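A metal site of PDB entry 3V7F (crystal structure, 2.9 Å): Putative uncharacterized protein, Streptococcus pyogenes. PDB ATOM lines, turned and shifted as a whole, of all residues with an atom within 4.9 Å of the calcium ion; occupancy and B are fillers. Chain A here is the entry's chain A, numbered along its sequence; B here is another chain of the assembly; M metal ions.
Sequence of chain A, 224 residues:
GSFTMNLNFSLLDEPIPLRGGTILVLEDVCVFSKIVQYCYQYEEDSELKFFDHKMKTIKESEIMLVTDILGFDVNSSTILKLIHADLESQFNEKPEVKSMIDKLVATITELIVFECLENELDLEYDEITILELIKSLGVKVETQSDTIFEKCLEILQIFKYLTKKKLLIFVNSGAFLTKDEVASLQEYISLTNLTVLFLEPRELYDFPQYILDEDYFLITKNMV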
ATOM      1  N   ASP A 126      18.009 -24.179 -20.071  1.00  0.00           N
ATOM      2  CA  ASP A 126      18.936 -23.096 -20.245  1.00  0.00           C
ATOM      3  C   ASP A 126      18.778 -22.448 -21.639  1.00  0.00           C
ATOM      4  O   ASP A 126      17.718 -21.869 -21.915  1.00  0.00           O
ATOM      5  CB  ASP A 126      20.368 -23.566 -19.950  1.00  0.00           C
ATOM      6  CG  ASP A 126      21.356 -22.399 -20.009  1.00  0.00           C
ATOM      7  OD1 ASP A 126      20.982 -21.291 -19.514  1.00  0.00           O
ATOM      8  OD2 ASP A 126      22.458 -22.555 -20.602  1.00  0.00           O
ATOM      9  N   GLU A 127      19.824 -22.476 -22.480  1.00  0.00           N
ATOM     10  CA  GLU A 127      19.684 -22.095 -23.893  1.00  0.00           C
ATOM     11  C   GLU A 127      20.291 -23.116 -24.851  1.00  0.00           C
ATOM     12  O   GLU A 127      20.908 -24.083 -24.402  1.00  0.00           O
ATOM     13  CB  GLU A 127      20.143 -20.663 -24.181  1.00  0.00           C
ATOM     14  CG  GLU A 127      21.384 -20.108 -23.527  1.00  0.00           C
ATOM     15  CD  GLU A 127      21.697 -18.693 -24.119  1.00  0.00           C
ATOM     16  OE1 GLU A 127      22.459 -17.908 -23.504  1.00  0.00           O
ATOM     17  OE2 GLU A 127      21.167 -18.356 -25.222  1.00  0.00           O
ATOM     18  N   ILE A 128      20.032 -22.952 -26.140  1.00  0.00           N
ATOM     19  CA  ILE A 128      20.749 -23.670 -27.182  1.00  0.00           C
ATOM     20  C   ILE A 128      21.584 -22.623 -27.893  1.00  0.00           C
ATOM     21  O   ILE A 128      21.061 -21.586 -28.342  1.00  0.00           O
ATOM     22  CB  ILE A 128      19.812 -24.314 -28.183  1.00  0.00           C
ATOM     23  CG1 ILE A 128      19.037 -25.453 -27.564  1.00  0.00           C
ATOM     24  CG2 ILE A 128      20.564 -24.869 -29.343  1.00  0.00           C
ATOM     25  CD1 ILE A 128      17.840 -25.927 -28.439  1.00  0.00           C
ATOM     26  N   GLU A 132      26.834 -24.926 -29.671  1.00  0.00           N
ATOM     27  CA  GLU A 132      26.334 -26.252 -29.341  1.00  0.00           C
ATOM     28  C   GLU A 132      25.832 -26.982 -30.597  1.00  0.00           C
ATOM     29  O   GLU A 132      25.958 -28.199 -30.718  1.00  0.00           O
ATOM     30  CB  GLU A 132      25.273 -26.208 -28.260  1.00  0.00           C
ATOM     31  CG  GLU A 132      25.680 -25.300 -27.200  1.00  0.00           C
ATOM     32  CD  GLU A 132      24.974 -25.524 -25.873  1.00  0.00           C
ATOM     33  OE1 GLU A 132      23.727 -25.276 -25.807  1.00  0.00           O
ATOM     34  OE2 GLU A 132      25.670 -25.895 -24.877  1.00  0.00           O
ATOM     35  N   SER B 136      21.391 -30.155 -25.498  1.00  0.00           N
ATOM     36  CA  SER B 136      22.025 -28.827 -25.556  1.00  0.00           C
ATOM     37  C   SER B 136      21.247 -27.755 -24.777  1.00  0.00           C
ATOM     38  O   SER B 136      21.828 -26.785 -24.266  1.00  0.00           O
ATOM     39  CB  SER B 136      22.263 -28.380 -26.998  1.00  0.00           C
ATOM     40  OG  SER B 136      23.112 -29.287 -27.684  1.00  0.00           O
ATOM     41  N   LEU B 137      19.928 -27.915 -24.693  1.00  0.00           N
ATOM     42  CA  LEU B 137      19.102 -26.959 -24.033  1.00  0.00           C
ATOM     43  C   LEU B 137      19.263 -27.095 -22.526  1.00  0.00           C
ATOM     44  O   LEU B 137      19.047 -26.142 -21.805  1.00  0.00           O
ATOM     45  CB  LEU B 137      17.674 -27.142 -24.442  1.00  0.00           C
ATOM     46  CG  LEU B 137      16.659 -26.196 -23.789  1.00  0.00           C
ATOM     47  CD1 LEU B 137      16.903 -24.691 -24.067  1.00  0.00           C
ATOM     48  CD2 LEU B 137      15.309 -26.598 -24.261  1.00  0.00           C
ATOM     49  N   GLY B 138      19.670 -28.247 -22.035  1.00  0.00           N
ATOM     50  CA  GLY B 138      20.056 -28.322 -20.643  1.00  0.00           C
ATOM     51  C   GLY B 138      18.863 -28.541 -19.766  1.00  0.00           C
ATOM     52  O   GLY B 138      18.847 -28.138 -18.602  1.00  0.00           O
HETATM   53 CA    CA M   1      22.957 -25.083 -23.495  1.00  0.00          CA
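O of Ser 136 of chain B is bound to the calcium ion (2.2 Å). The calcium ion is bound by the side-chain carboxylate (OE1) of Glu 132 (2.4 Å). The calcium ion is bound by the backbone carbonyl oxygen (O) of Glu 127, at 2.5 Å. The calcium ion has three donor atoms within binding distance.
O of Leu 137 of chain B lies within hydrogen-bond range of N of Asp 126.
Merely in contact with the calcium ion: Asp 126 (3.9 Å). Of the 7 residues printed, 4 come within 4 Å of the calcium ion.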
